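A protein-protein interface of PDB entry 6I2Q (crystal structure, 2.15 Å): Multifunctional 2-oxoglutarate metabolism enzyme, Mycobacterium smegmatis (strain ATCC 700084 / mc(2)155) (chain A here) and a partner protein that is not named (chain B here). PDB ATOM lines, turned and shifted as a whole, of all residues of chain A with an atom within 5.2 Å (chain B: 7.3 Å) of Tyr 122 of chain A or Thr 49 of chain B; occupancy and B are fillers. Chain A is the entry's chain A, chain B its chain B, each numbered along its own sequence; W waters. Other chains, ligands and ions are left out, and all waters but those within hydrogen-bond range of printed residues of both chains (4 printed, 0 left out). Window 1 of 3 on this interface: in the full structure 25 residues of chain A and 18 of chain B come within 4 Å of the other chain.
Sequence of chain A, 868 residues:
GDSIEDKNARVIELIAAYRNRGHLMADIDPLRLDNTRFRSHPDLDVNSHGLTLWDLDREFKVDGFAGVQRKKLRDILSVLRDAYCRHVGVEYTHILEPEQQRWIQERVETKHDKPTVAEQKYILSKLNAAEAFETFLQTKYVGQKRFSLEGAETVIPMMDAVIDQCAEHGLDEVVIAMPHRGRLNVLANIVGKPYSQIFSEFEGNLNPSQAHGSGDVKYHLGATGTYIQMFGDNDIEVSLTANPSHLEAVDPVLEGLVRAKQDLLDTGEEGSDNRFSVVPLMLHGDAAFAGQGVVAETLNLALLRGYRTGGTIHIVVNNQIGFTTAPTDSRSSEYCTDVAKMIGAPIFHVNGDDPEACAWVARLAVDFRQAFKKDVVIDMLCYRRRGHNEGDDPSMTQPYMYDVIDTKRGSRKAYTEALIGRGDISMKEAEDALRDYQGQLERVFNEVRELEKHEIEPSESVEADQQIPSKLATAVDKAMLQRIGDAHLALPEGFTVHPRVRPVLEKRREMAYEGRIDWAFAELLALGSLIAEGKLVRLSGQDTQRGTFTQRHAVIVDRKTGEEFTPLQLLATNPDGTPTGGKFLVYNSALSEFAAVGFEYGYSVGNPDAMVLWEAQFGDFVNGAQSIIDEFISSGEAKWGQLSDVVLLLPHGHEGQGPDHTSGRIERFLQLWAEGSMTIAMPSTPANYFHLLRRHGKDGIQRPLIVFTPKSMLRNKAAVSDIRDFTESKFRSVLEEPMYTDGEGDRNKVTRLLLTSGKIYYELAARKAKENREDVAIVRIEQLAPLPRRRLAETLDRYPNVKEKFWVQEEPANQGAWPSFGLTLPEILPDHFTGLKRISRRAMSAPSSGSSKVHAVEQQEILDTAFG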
ATOM      1  N   VAL A 117       1.107 -12.676 -11.553  1.00  0.00           N
ATOM      2  CA  VAL A 117       1.891 -13.715 -12.221  1.00  0.00           C
ATOM      3  C   VAL A 117       1.438 -13.777 -13.694  1.00  0.00           C
ATOM      4  O   VAL A 117       2.284 -13.840 -14.586  1.00  0.00           O
ATOM      5  CB  VAL A 117       1.795 -15.096 -11.505  1.00  0.00           C
ATOM      6  CG1 VAL A 117       2.542 -16.179 -12.282  1.00  0.00           C
ATOM      7  CG2 VAL A 117       2.342 -15.009 -10.084  1.00  0.00           C
ATOM      8  N   ALA A 118       0.117 -13.687 -13.941  1.00  0.00           N
ATOM      9  CA  ALA A 118      -0.435 -13.734 -15.295  1.00  0.00           C
ATOM     10  C   ALA A 118       0.074 -12.567 -16.145  1.00  0.00           C
ATOM     11  O   ALA A 118       0.395 -12.771 -17.316  1.00  0.00           O
ATOM     12  CB  ALA A 118      -1.954 -13.740 -15.251  1.00  0.00           C
ATOM     13  N   GLU A 119       0.221 -11.368 -15.545  1.00  0.00           N
ATOM     14  CA  GLU A 119       0.746 -10.203 -16.277  1.00  0.00           C
ATOM     15  C   GLU A 119       2.239 -10.391 -16.594  1.00  0.00           C
ATOM     16  O   GLU A 119       2.667 -10.070 -17.704  1.00  0.00           O
ATOM     17  CB  GLU A 119       0.502  -8.893 -15.509  1.00  0.00           C
ATOM     18  CG  GLU A 119      -0.946  -8.444 -15.605  1.00  0.00           C
ATOM     19  CD  GLU A 119      -1.447  -7.474 -14.551  1.00  0.00           C
ATOM     20  OE1 GLU A 119      -2.553  -6.926 -14.749  1.00  0.00           O
ATOM     21  OE2 GLU A 119      -0.750  -7.259 -13.532  1.00  0.00           O
ATOM     22  N   GLN A 120       3.012 -10.935 -15.636  1.00  0.00           N
ATOM     23  CA  GLN A 120       4.445 -11.220 -15.805  1.00  0.00           C
ATOM     24  C   GLN A 120       4.647 -12.279 -16.902  1.00  0.00           C
ATOM     25  O   GLN A 120       5.455 -12.080 -17.806  1.00  0.00           O
ATOM     26  CB  GLN A 120       5.077 -11.688 -14.479  1.00  0.00           C
ATOM     27  CG  GLN A 120       5.056 -10.620 -13.377  1.00  0.00           C
ATOM     28  CD  GLN A 120       5.582 -11.163 -12.071  1.00  0.00           C
ATOM     29  OE1 GLN A 120       5.069 -12.144 -11.503  1.00  0.00           O
ATOM     30  NE2 GLN A 120       6.606 -10.518 -11.548  1.00  0.00           N
ATOM     31  N   LYS A 121       3.859 -13.364 -16.857  1.00  0.00           N
ATOM     32  CA  LYS A 121       3.896 -14.432 -17.865  1.00  0.00           C
ATOM     33  C   LYS A 121       3.534 -13.902 -19.266  1.00  0.00           C
ATOM     34  O   LYS A 121       4.161 -14.298 -20.243  1.00  0.00           O
ATOM     35  CB  LYS A 121       2.952 -15.569 -17.483  1.00  0.00           C
ATOM     36  CG  LYS A 121       3.471 -16.451 -16.368  1.00  0.00           C
ATOM     37  CD  LYS A 121       2.392 -17.448 -15.976  1.00  0.00           C
ATOM     38  CE  LYS A 121       2.907 -18.560 -15.112  1.00  0.00           C
ATOM     39  NZ  LYS A 121       1.804 -19.473 -14.731  1.00  0.00           N
ATOM     40  N   TYR A 122       2.569 -12.960 -19.347  1.00  0.00           N
ATOM     41  CA  TYR A 122       2.149 -12.349 -20.608  1.00  0.00           C
ATOM     42  C   TYR A 122       3.299 -11.497 -21.212  1.00  0.00           C
ATOM     43  O   TYR A 122       3.539 -11.555 -22.421  1.00  0.00           O
ATOM     44  CB  TYR A 122       0.856 -11.520 -20.412  1.00  0.00           C
ATOM     45  CG  TYR A 122       0.403 -10.855 -21.694  1.00  0.00           C
ATOM     46  CD1 TYR A 122      -0.163 -11.601 -22.730  1.00  0.00           C
ATOM     47  CD2 TYR A 122       0.611  -9.494 -21.905  1.00  0.00           C
ATOM     48  CE1 TYR A 122      -0.512 -11.005 -23.941  1.00  0.00           C
ATOM     49  CE2 TYR A 122       0.256  -8.887 -23.104  1.00  0.00           C
ATOM     50  CZ  TYR A 122      -0.312  -9.645 -24.118  1.00  0.00           C
ATOM     51  OH  TYR A 122      -0.660  -9.047 -25.297  1.00  0.00           O
ATOM     52  N   ILE A 123       3.991 -10.705 -20.368  1.00  0.00           N
ATOM     53  CA  ILE A 123       5.140  -9.907 -20.785  1.00  0.00           C
ATOM     54  C   ILE A 123       6.235 -10.881 -21.296  1.00  0.00           C
ATOM     55  O   ILE A 123       6.821 -10.645 -22.357  1.00  0.00           O
ATOM     56  CB  ILE A 123       5.649  -8.995 -19.629  1.00  0.00           C
ATOM     57  CG1 ILE A 123       4.697  -7.817 -19.380  1.00  0.00           C
ATOM     58  CG2 ILE A 123       7.100  -8.520 -19.865  1.00  0.00           C
ATOM     59  CD1 ILE A 123       5.000  -7.007 -18.027  1.00  0.00           C
ATOM     60  N   LEU A 124       6.485 -11.964 -20.552  1.00  0.00           N
ATOM     61  CA  LEU A 124       7.468 -12.979 -20.956  1.00  0.00           C
ATOM     62  C   LEU A 124       7.054 -13.620 -22.304  1.00  0.00           C
ATOM     63  O   LEU A 124       7.917 -13.798 -23.163  1.00  0.00           O
ATOM     64  CB  LEU A 124       7.670 -14.042 -19.865  1.00  0.00           C
ATOM     65  CG  LEU A 124       8.739 -15.123 -20.122  1.00  0.00           C
ATOM     66  CD1 LEU A 124      10.087 -14.506 -20.542  1.00  0.00           C
ATOM     67  CD2 LEU A 124       8.908 -15.999 -18.908  1.00  0.00           C
ATOM     68  N   SER A 125       5.741 -13.858 -22.523  1.00  0.00           N
ATOM     69  CA  SER A 125       5.237 -14.393 -23.799  1.00  0.00           C
ATOM     70  C   SER A 125       5.556 -13.414 -24.960  1.00  0.00           C
ATOM     71  O   SER A 125       5.887 -13.876 -26.039  1.00  0.00           O
ATOM     72  CB  SER A 125       3.743 -14.717 -23.718  1.00  0.00           C
ATOM     73  OG  SER A 125       2.890 -13.619 -23.987  1.00  0.00           O
ATOM     74  N   LYS A 126       5.536 -12.083 -24.707  1.00  0.00           N
ATOM     75  CA  LYS A 126       5.860 -11.070 -25.730  1.00  0.00           C
ATOM     76  C   LYS A 126       7.363 -11.007 -25.995  1.00  0.00           C
ATOM     77  O   LYS A 126       7.761 -10.725 -27.123  1.00  0.00           O
ATOM     78  CB  LYS A 126       5.298  -9.675 -25.396  1.00  0.00           C
ATOM     79  CG  LYS A 126       3.771  -9.559 -25.574  1.00  0.00           C
ATOM     80  CD  LYS A 126       3.287  -9.697 -27.033  1.00  0.00           C
ATOM     81  CE  LYS A 126       1.842 -10.146 -27.059  1.00  0.00           C
ATOM     82  NZ  LYS A 126       1.449 -10.816 -28.334  1.00  0.00           N
ATOM     83  N   ASP A 160       3.024  -3.014 -26.824  1.00  0.00           N
ATOM     84  CA  ASP A 160       1.842  -3.806 -26.528  1.00  0.00           C
ATOM     85  C   ASP A 160       1.051  -3.179 -25.344  1.00  0.00           C
ATOM     86  O   ASP A 160      -0.172  -3.081 -25.408  1.00  0.00           O
ATOM     87  CB  ASP A 160       2.266  -5.257 -26.239  1.00  0.00           C
ATOM     88  CG  ASP A 160       1.091  -6.204 -26.153  1.00  0.00           C
ATOM     89  OD1 ASP A 160       0.499  -6.305 -25.076  1.00  0.00           O
ATOM     90  OD2 ASP A 160       0.763  -6.818 -27.163  1.00  0.00           O
ATOM     91  N   TYR A 227      -6.118  -5.313 -32.697  1.00  0.00           N
ATOM     92  CA  TYR A 227      -5.538  -5.710 -31.428  1.00  0.00           C
ATOM     93  C   TYR A 227      -6.677  -6.111 -30.464  1.00  0.00           C
ATOM     94  O   TYR A 227      -7.650  -5.359 -30.312  1.00  0.00           O
ATOM     95  CB  TYR A 227      -4.677  -4.583 -30.842  1.00  0.00           C
ATOM     96  CG  TYR A 227      -4.026  -4.941 -29.528  1.00  0.00           C
ATOM     97  CD1 TYR A 227      -2.706  -5.393 -29.480  1.00  0.00           C
ATOM     98  CD2 TYR A 227      -4.718  -4.807 -28.321  1.00  0.00           C
ATOM     99  CE1 TYR A 227      -2.103  -5.731 -28.268  1.00  0.00           C
ATOM    100  CE2 TYR A 227      -4.123  -5.138 -27.108  1.00  0.00           C
ATOM    101  CZ  TYR A 227      -2.818  -5.602 -27.086  1.00  0.00           C
ATOM    102  OH  TYR A 227      -2.232  -5.902 -25.880  1.00  0.00           O
ATOM    103  N   MET A 230      -5.849  -8.974 -23.840  1.00  0.00           N
ATOM    104  CA  MET A 230      -5.632 -10.262 -23.199  1.00  0.00           C
ATOM    105  C   MET A 230      -6.450 -10.362 -21.901  1.00  0.00           C
ATOM    106  O   MET A 230      -7.029 -11.407 -21.621  1.00  0.00           O
ATOM    107  CB  MET A 230      -4.123 -10.444 -22.919  1.00  0.00           C
ATOM    108  CG  MET A 230      -3.785 -11.709 -22.178  1.00  0.00           C
ATOM    109  SD  MET A 230      -4.011 -13.195 -23.178  1.00  0.00           S
ATOM    110  CE  MET A 230      -4.032 -14.426 -21.864  1.00  0.00           C
ATOM    111  N   PHE A 231      -6.485  -9.294 -21.112  1.00  0.00           N
ATOM    112  CA  PHE A 231      -7.164  -9.316 -19.819  1.00  0.00           C
ATOM    113  C   PHE A 231      -8.403  -8.413 -19.766  1.00  0.00           C
ATOM    114  O   PHE A 231      -9.127  -8.441 -18.770  1.00  0.00           O
ATOM    115  CB  PHE A 231      -6.169  -8.937 -18.701  1.00  0.00           C
ATOM    116  CG  PHE A 231      -4.985  -9.884 -18.648  1.00  0.00           C
ATOM    117  CD1 PHE A 231      -3.721  -9.466 -19.051  1.00  0.00           C
ATOM    118  CD2 PHE A 231      -5.149 -11.210 -18.256  1.00  0.00           C
ATOM    119  CE1 PHE A 231      -2.633 -10.345 -19.023  1.00  0.00           C
ATOM    120  CE2 PHE A 231      -4.064 -12.091 -18.241  1.00  0.00           C
ATOM    121  CZ  PHE A 231      -2.812 -11.652 -18.618  1.00  0.00           C
ATOM    122  N   ARG B  37      -1.232 -23.886 -30.688  1.00  0.00           N
ATOM    123  CA  ARG B  37      -0.639 -23.211 -31.842  1.00  0.00           C
ATOM    124  C   ARG B  37       0.060 -24.198 -32.821  1.00  0.00           C
ATOM    125  O   ARG B  37       0.435 -23.789 -33.926  1.00  0.00           O
ATOM    126  CB  ARG B  37       0.324 -22.098 -31.394  1.00  0.00           C
ATOM    127  CG  ARG B  37       0.542 -21.059 -32.479  1.00  0.00           C
ATOM    128  CD  ARG B  37       1.158 -19.790 -31.969  1.00  0.00           C
ATOM    129  NE  ARG B  37       1.209 -18.789 -33.029  1.00  0.00           N
ATOM    130  CZ  ARG B  37       2.327 -18.275 -33.528  1.00  0.00           C
ATOM    131  NH1 ARG B  37       3.507 -18.633 -33.039  1.00  0.00           N
ATOM    132  NH2 ARG B  37       2.272 -17.385 -34.509  1.00  0.00           N
ATOM    133  N   LEU B  45      -5.404 -22.861 -32.870  1.00  0.00           N
ATOM    134  CA  LEU B  45      -5.642 -21.483 -32.438  1.00  0.00           C
ATOM    135  C   LEU B  45      -4.380 -20.650 -32.702  1.00  0.00           C
ATOM    136  O   LEU B  45      -3.447 -20.611 -31.896  1.00  0.00           O
ATOM    137  CB  LEU B  45      -6.106 -21.445 -30.966  1.00  0.00           C
ATOM    138  CG  LEU B  45      -7.456 -22.138 -30.683  1.00  0.00           C
ATOM    139  CD1 LEU B  45      -7.767 -22.156 -29.203  1.00  0.00           C
ATOM    140  CD2 LEU B  45      -8.604 -21.485 -31.453  1.00  0.00           C
ATOM    141  N   ASP B  46      -4.366 -20.011 -33.882  1.00  0.00           N
ATOM    142  CA  ASP B  46      -3.234 -19.288 -34.448  1.00  0.00           C
ATOM    143  C   ASP B  46      -3.046 -17.843 -33.934  1.00  0.00           C
ATOM    144  O   ASP B  46      -3.347 -16.877 -34.642  1.00  0.00           O
ATOM    145  CB  ASP B  46      -3.347 -19.282 -35.985  1.00  0.00           C
ATOM    146  CG  ASP B  46      -2.057 -19.022 -36.728  1.00  0.00           C
ATOM    147  OD1 ASP B  46      -1.005 -18.899 -36.069  1.00  0.00           O
ATOM    148  OD2 ASP B  46      -2.098 -18.938 -37.969  1.00  0.00           O
ATOM    149  N   ASP B  47      -2.447 -17.715 -32.742  1.00  0.00           N
ATOM    150  CA  ASP B  47      -2.027 -16.445 -32.134  1.00  0.00           C
ATOM    151  C   ASP B  47      -0.808 -16.720 -31.258  1.00  0.00           C
ATOM    152  O   ASP B  47      -0.760 -17.763 -30.598  1.00  0.00           O
ATOM    153  CB  ASP B  47      -3.151 -15.773 -31.331  1.00  0.00           C
ATOM    154  CG  ASP B  47      -2.849 -14.320 -31.046  1.00  0.00           C
ATOM    155  OD1 ASP B  47      -3.152 -13.472 -31.913  1.00  0.00           O
ATOM    156  OD2 ASP B  47      -2.275 -14.032 -29.969  1.00  0.00           O
ATOM    157  N   VAL B  48       0.169 -15.792 -31.239  1.00  0.00           N
ATOM    158  CA  VAL B  48       1.416 -15.913 -30.445  1.00  0.00           C
ATOM    159  C   VAL B  48       1.130 -16.083 -28.940  1.00  0.00           C
ATOM    160  O   VAL B  48       1.974 -16.643 -28.235  1.00  0.00           O
ATOM    161  CB  VAL B  48       2.423 -14.748 -30.675  1.00  0.00           C
ATOM    162  CG1 VAL B  48       3.049 -14.816 -32.062  1.00  0.00           C
ATOM    163  CG2 VAL B  48       1.780 -13.399 -30.439  1.00  0.00           C
ATOM    164  N   THR B  49      -0.065 -15.649 -28.463  1.00  0.00           N
ATOM    165  CA  THR B  49      -0.494 -15.792 -27.059  1.00  0.00           C
ATOM    166  C   THR B  49      -0.807 -17.241 -26.701  1.00  0.00           C
ATOM    167  O   THR B  49      -0.875 -17.562 -25.519  1.00  0.00           O
ATOM    168  CB  THR B  49      -1.724 -14.909 -26.748  1.00  0.00           C
ATOM    169  OG1 THR B  49      -2.812 -15.258 -27.619  1.00  0.00           O
ATOM    170  CG2 THR B  49      -1.411 -13.424 -26.817  1.00  0.00           C
ATOM    171  N   VAL B  50      -1.047 -18.100 -27.716  1.00  0.00           N
ATOM    172  CA  VAL B  50      -1.364 -19.521 -27.557  1.00  0.00           C
ATOM    173  C   VAL B  50      -0.061 -20.333 -27.675  1.00  0.00           C
ATOM    174  O   VAL B  50       0.734 -20.116 -28.597  1.00  0.00           O
ATOM    175  CB  VAL B  50      -2.435 -19.980 -28.594  1.00  0.00           C
ATOM    176  CG1 VAL B  50      -2.790 -21.463 -28.434  1.00  0.00           C
ATOM    177  CG2 VAL B  50      -3.695 -19.112 -28.513  1.00  0.00           C
ATOM    178  N   SER B  51       0.159 -21.268 -26.743  1.00  0.00           N
ATOM    179  CA  SER B  51       1.358 -22.087 -26.783  1.00  0.00           C
ATOM    180  C   SER B  51       1.153 -23.241 -27.762  1.00  0.00           C
ATOM    181  O   SER B  51       0.008 -23.673 -27.975  1.00  0.00           O
ATOM    182  CB  SER B  51       1.717 -22.586 -25.387  1.00  0.00           C
ATOM    183  OG  SER B  51       1.985 -21.496 -24.516  1.00  0.00           O
ATOM    184  N   HIS B  54      -1.146 -26.291 -25.702  1.00  0.00           N
ATOM    185  CA  HIS B  54      -1.754 -25.353 -24.754  1.00  0.00           C
ATOM    186  C   HIS B  54      -2.824 -26.004 -23.876  1.00  0.00           C
ATOM    187  O   HIS B  54      -2.707 -25.984 -22.646  1.00  0.00           O
ATOM    188  CB  HIS B  54      -2.353 -24.152 -25.528  1.00  0.00           C
ATOM    189  CG  HIS B  54      -2.653 -22.947 -24.687  1.00  0.00           C
ATOM    190  ND1 HIS B  54      -1.977 -21.753 -24.875  1.00  0.00           N
ATOM    191  CD2 HIS B  54      -3.542 -22.789 -23.676  1.00  0.00           C
ATOM    192  CE1 HIS B  54      -2.479 -20.910 -23.988  1.00  0.00           C
ATOM    193  NE2 HIS B  54      -3.415 -21.492 -23.237  1.00  0.00           N
ATOM    194  N   SER B  71       0.886 -24.616 -20.872  1.00  0.00           N
ATOM    195  CA  SER B  71       0.955 -23.368 -21.629  1.00  0.00           C
ATOM    196  C   SER B  71       1.573 -22.258 -20.789  1.00  0.00           C
ATOM    197  O   SER B  71       1.574 -22.343 -19.560  1.00  0.00           O
ATOM    198  CB  SER B  71      -0.438 -22.954 -22.080  1.00  0.00           C
ATOM    199  OG  SER B  71      -1.169 -22.279 -21.070  1.00  0.00           O
ATOM    200  N   LEU B  72       2.076 -21.214 -21.448  1.00  0.00           N
ATOM    201  CA  LEU B  72       2.648 -20.072 -20.758  1.00  0.00           C
ATOM    202  C   LEU B  72       1.556 -19.143 -20.212  1.00  0.00           C
ATOM    203  O   LEU B  72       1.687 -18.684 -19.076  1.00  0.00           O
ATOM    204  CB  LEU B  72       3.597 -19.292 -21.698  1.00  0.00           C
ATOM    205  CG  LEU B  72       4.325 -18.042 -21.177  1.00  0.00           C
ATOM    206  CD1 LEU B  72       5.004 -18.269 -19.802  1.00  0.00           C
ATOM    207  CD2 LEU B  72       5.358 -17.601 -22.170  1.00  0.00           C
ATOM    208  N   ASN B  73       0.510 -18.836 -21.011  1.00  0.00           N
ATOM    209  CA  ASN B  73      -0.510 -17.859 -20.588  1.00  0.00           C
ATOM    210  C   ASN B  73      -1.728 -18.500 -19.863  1.00  0.00           C
ATOM    211  O   ASN B  73      -2.599 -17.769 -19.399  1.00  0.00           O
ATOM    212  CB  ASN B  73      -0.971 -16.990 -21.775  1.00  0.00           C
ATOM    213  CG  ASN B  73       0.064 -15.990 -22.239  1.00  0.00           C
ATOM    214  OD1 ASN B  73       0.621 -15.211 -21.452  1.00  0.00           O
ATOM    215  ND2 ASN B  73       0.330 -15.971 -23.542  1.00  0.00           N
ATOM    216  N   GLY B  74      -1.742 -19.830 -19.715  1.00  0.00           N
ATOM    217  CA  GLY B  74      -2.806 -20.518 -18.993  1.00  0.00           C
ATOM    218  C   GLY B  74      -4.143 -20.626 -19.706  1.00  0.00           C
ATOM    219  O   GLY B  74      -4.268 -20.265 -20.875  1.00  0.00           O
ATOM    220  N   ILE B  95      -8.201 -19.172 -24.219  1.00  0.00           N
ATOM    221  CA  ILE B  95      -6.915 -19.793 -24.591  1.00  0.00           C
ATOM    222  C   ILE B  95      -6.144 -18.703 -25.325  1.00  0.00           C
ATOM    223  O   ILE B  95      -6.466 -18.369 -26.467  1.00  0.00           O
ATOM    224  CB  ILE B  95      -7.094 -21.121 -25.399  1.00  0.00           C
ATOM    225  CG1 ILE B  95      -7.714 -22.236 -24.509  1.00  0.00           C
ATOM    226  CG2 ILE B  95      -5.766 -21.603 -26.010  1.00  0.00           C
ATOM    227  CD1 ILE B  95      -8.459 -23.339 -25.283  1.00  0.00           C
ATOM    228  N   GLY B  96      -5.195 -18.087 -24.621  1.00  0.00           N
ATOM    229  CA  GLY B  96      -4.494 -16.916 -25.126  1.00  0.00           C
ATOM    230  C   GLY B  96      -5.519 -15.802 -25.275  1.00  0.00           C
ATOM    231  O   GLY B  96      -6.415 -15.680 -24.433  1.00  0.00           O
ATOM    232  N   LYS B  97      -5.480 -15.054 -26.403  1.00  0.00           N
ATOM    233  CA  LYS B  97      -6.458 -13.993 -26.661  1.00  0.00           C
ATOM    234  C   LYS B  97      -7.805 -14.559 -27.163  1.00  0.00           C
ATOM    235  O   LYS B  97      -8.788 -13.823 -27.216  1.00  0.00           O
ATOM    236  CB  LYS B  97      -5.895 -12.956 -27.642  1.00  0.00           C
ATOM    237  CG  LYS B  97      -4.919 -12.021 -26.942  1.00  0.00           C
ATOM    238  CD  LYS B  97      -4.202 -11.119 -27.886  1.00  0.00           C
ATOM    239  CE  LYS B  97      -3.357 -10.124 -27.127  1.00  0.00           C
ATOM    240  NZ  LYS B  97      -2.609  -9.268 -28.068  1.00  0.00           N
ATOM    241  N   PHE B  98      -7.869 -15.852 -27.497  1.00  0.00           N
ATOM    242  CA  PHE B  98      -9.120 -16.455 -27.967  1.00  0.00           C
ATOM    243  C   PHE B  98     -10.133 -16.681 -26.839  1.00  0.00           C
ATOM    244  O   PHE B  98      -9.766 -17.145 -25.762  1.00  0.00           O
ATOM    245  CB  PHE B  98      -8.874 -17.806 -28.672  1.00  0.00           C
ATOM    246  CG  PHE B  98      -8.121 -17.715 -29.971  1.00  0.00           C
ATOM    247  CD1 PHE B  98      -6.737 -17.840 -30.001  1.00  0.00           C
ATOM    248  CD2 PHE B  98      -8.797 -17.547 -31.176  1.00  0.00           C
ATOM    249  CE1 PHE B  98      -6.035 -17.782 -31.216  1.00  0.00           C
ATOM    250  CE2 PHE B  98      -8.096 -17.508 -32.393  1.00  0.00           C
ATOM    251  CZ  PHE B  98      -6.719 -17.615 -32.401  1.00  0.00           C
HETATM  252  O   HOH W   1      -0.236  -8.359 -29.096  1.00  0.00           O
HETATM  253  O   HOH W   2      -1.185 -11.273 -29.665  1.00  0.00           O
HETATM  254  O   HOH W   3      -0.218 -19.592 -16.655  1.00  0.00           O
HETATM  255  O   HOH W   4      -0.477 -14.749 -18.951  1.00  0.00           O
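Water W1 lies within hydrogen-bond range of the side-chain carboxylate (OD2) of Asp 160 of chain A (2.7 Å), the side-chain amino group (NZ) of Lys 97 of chain B (2.7 Å) and the side-chain amino group (NZ) of Lys 126 of chain A (3.1 Å). Water W4 lies within hydrogen-bond range of the backbone carbonyl oxygen of Ala 118 of chain A (2.7 Å) and the side-chain amide oxygen of Asn 73 of chain B (2.8 Å). Water W3 lies within hydrogen-bond range of NZ of Lys 121 of chain A (2.8 Å), O of Leu 72 of chain B (3.2 Å) and N of Gly 74 of chain B (3.4 Å). Water W2 lies within hydrogen-bond range of NZ of Lys 97 of chain B, OD2 of Asp 47 of chain B and NZ of Lys 126 of chain A.
Among the printed residues, pairs that only touch across the chains: Lys 126 of chain A with Val 48 of chain B, Tyr 122 of chain A with Asn 73 of chain B, Lys 121 of chain A with Leu 72 of chain B, Ser 125 of chain A with Asn 73 of chain B, Tyr 227 of chain A with Lys 97 of chain B, Ser 125 of chain A with Leu 72 of chain B, Lys 121 of chain A with Asn 73 of chain B, Tyr 122 of chain A with Thr 49 of chain B and Met 230 of chain A with Asn 73 of chain B.
NZ of Lys 97 of chain B lies within hydrogen-bond range of OH of Tyr 122 of chain A, at 3.4 Å. The backbone carbonyl oxygen (O) of Gly 96 of chain B sits close to the side-chain sulfur (SD) of Met 230 of chain A (3.7 Å).
Of the printed residues of chain B, Tyr 122 of chain A touches Thr 49, Asn 73 and Lys 97. Of the printed residues of chain B, Tyr 227 of chain A touches Lys 97 (3.6 Å). Thr 49 of chain B touches just one residue of chain A: Tyr 122. Of the printed residues of chain A, Asn 73 of chain B touches Lys 121 (3.9 Å), Tyr 122 (3.4 Å), Ser 125 (3.5 Å) and Met 230 (3.99 Å). Of the printed residues of chain A, Lys 97 of chain B touches Tyr 122 (3.4 Å) and Tyr 227 (3.6 Å). The nearest residue of chain A that does not touch Thr 49 of chain B is Lys 126 of chain A (4.2 Å). The nearest printed residue of chain B that does not touch Met 230 of chain A is Lys 97 of chain B (4.002 Å).
O of Tyr 122 of chain A is in hydrogen-bond range of OG of Ser 125 of chain A. OH of Tyr 227 of chain A is in hydrogen-bond range of OD1 of Asp 160 of chain A. The side-chain carboxylate (OD2) of Asp 47 of chain B lies within hydrogen-bond range of the side-chain hydroxyl (OG1) of Thr 49 of chain B (2.7 Å). The side-chain amide nitrogen (ND2) of Asn 73 of chain B sits at hydrogen-bond distance from the backbone carbonyl oxygen (O) of Thr 49 of chain B (2.8 Å). The backbone NH (N) of Lys 97 of chain B is in hydrogen-bond range of the side-chain hydroxyl (OG1) of Thr 49 of chain B. The side-chain hydroxyl (OG) of Ser 51 of chain B sits at hydrogen-bond distance from the backbone NH (N) of Leu 72 of chain B.
Printed residues of chain B that touch a printed residue of chain A: Val 48, Thr 49, Leu 72, Asn 73, Gly 96 and Lys 97. Hydrophobic or aromatic side chains of chain B that line the printed part of chain A: Val 48 and Leu 72. Hydrophobic or aromatic side chains of chain A within 4 Å of the printed part of chain B: Tyr 122, Tyr 227 and Met 230. Among the printed residues, 11 pairs touch across the chains.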
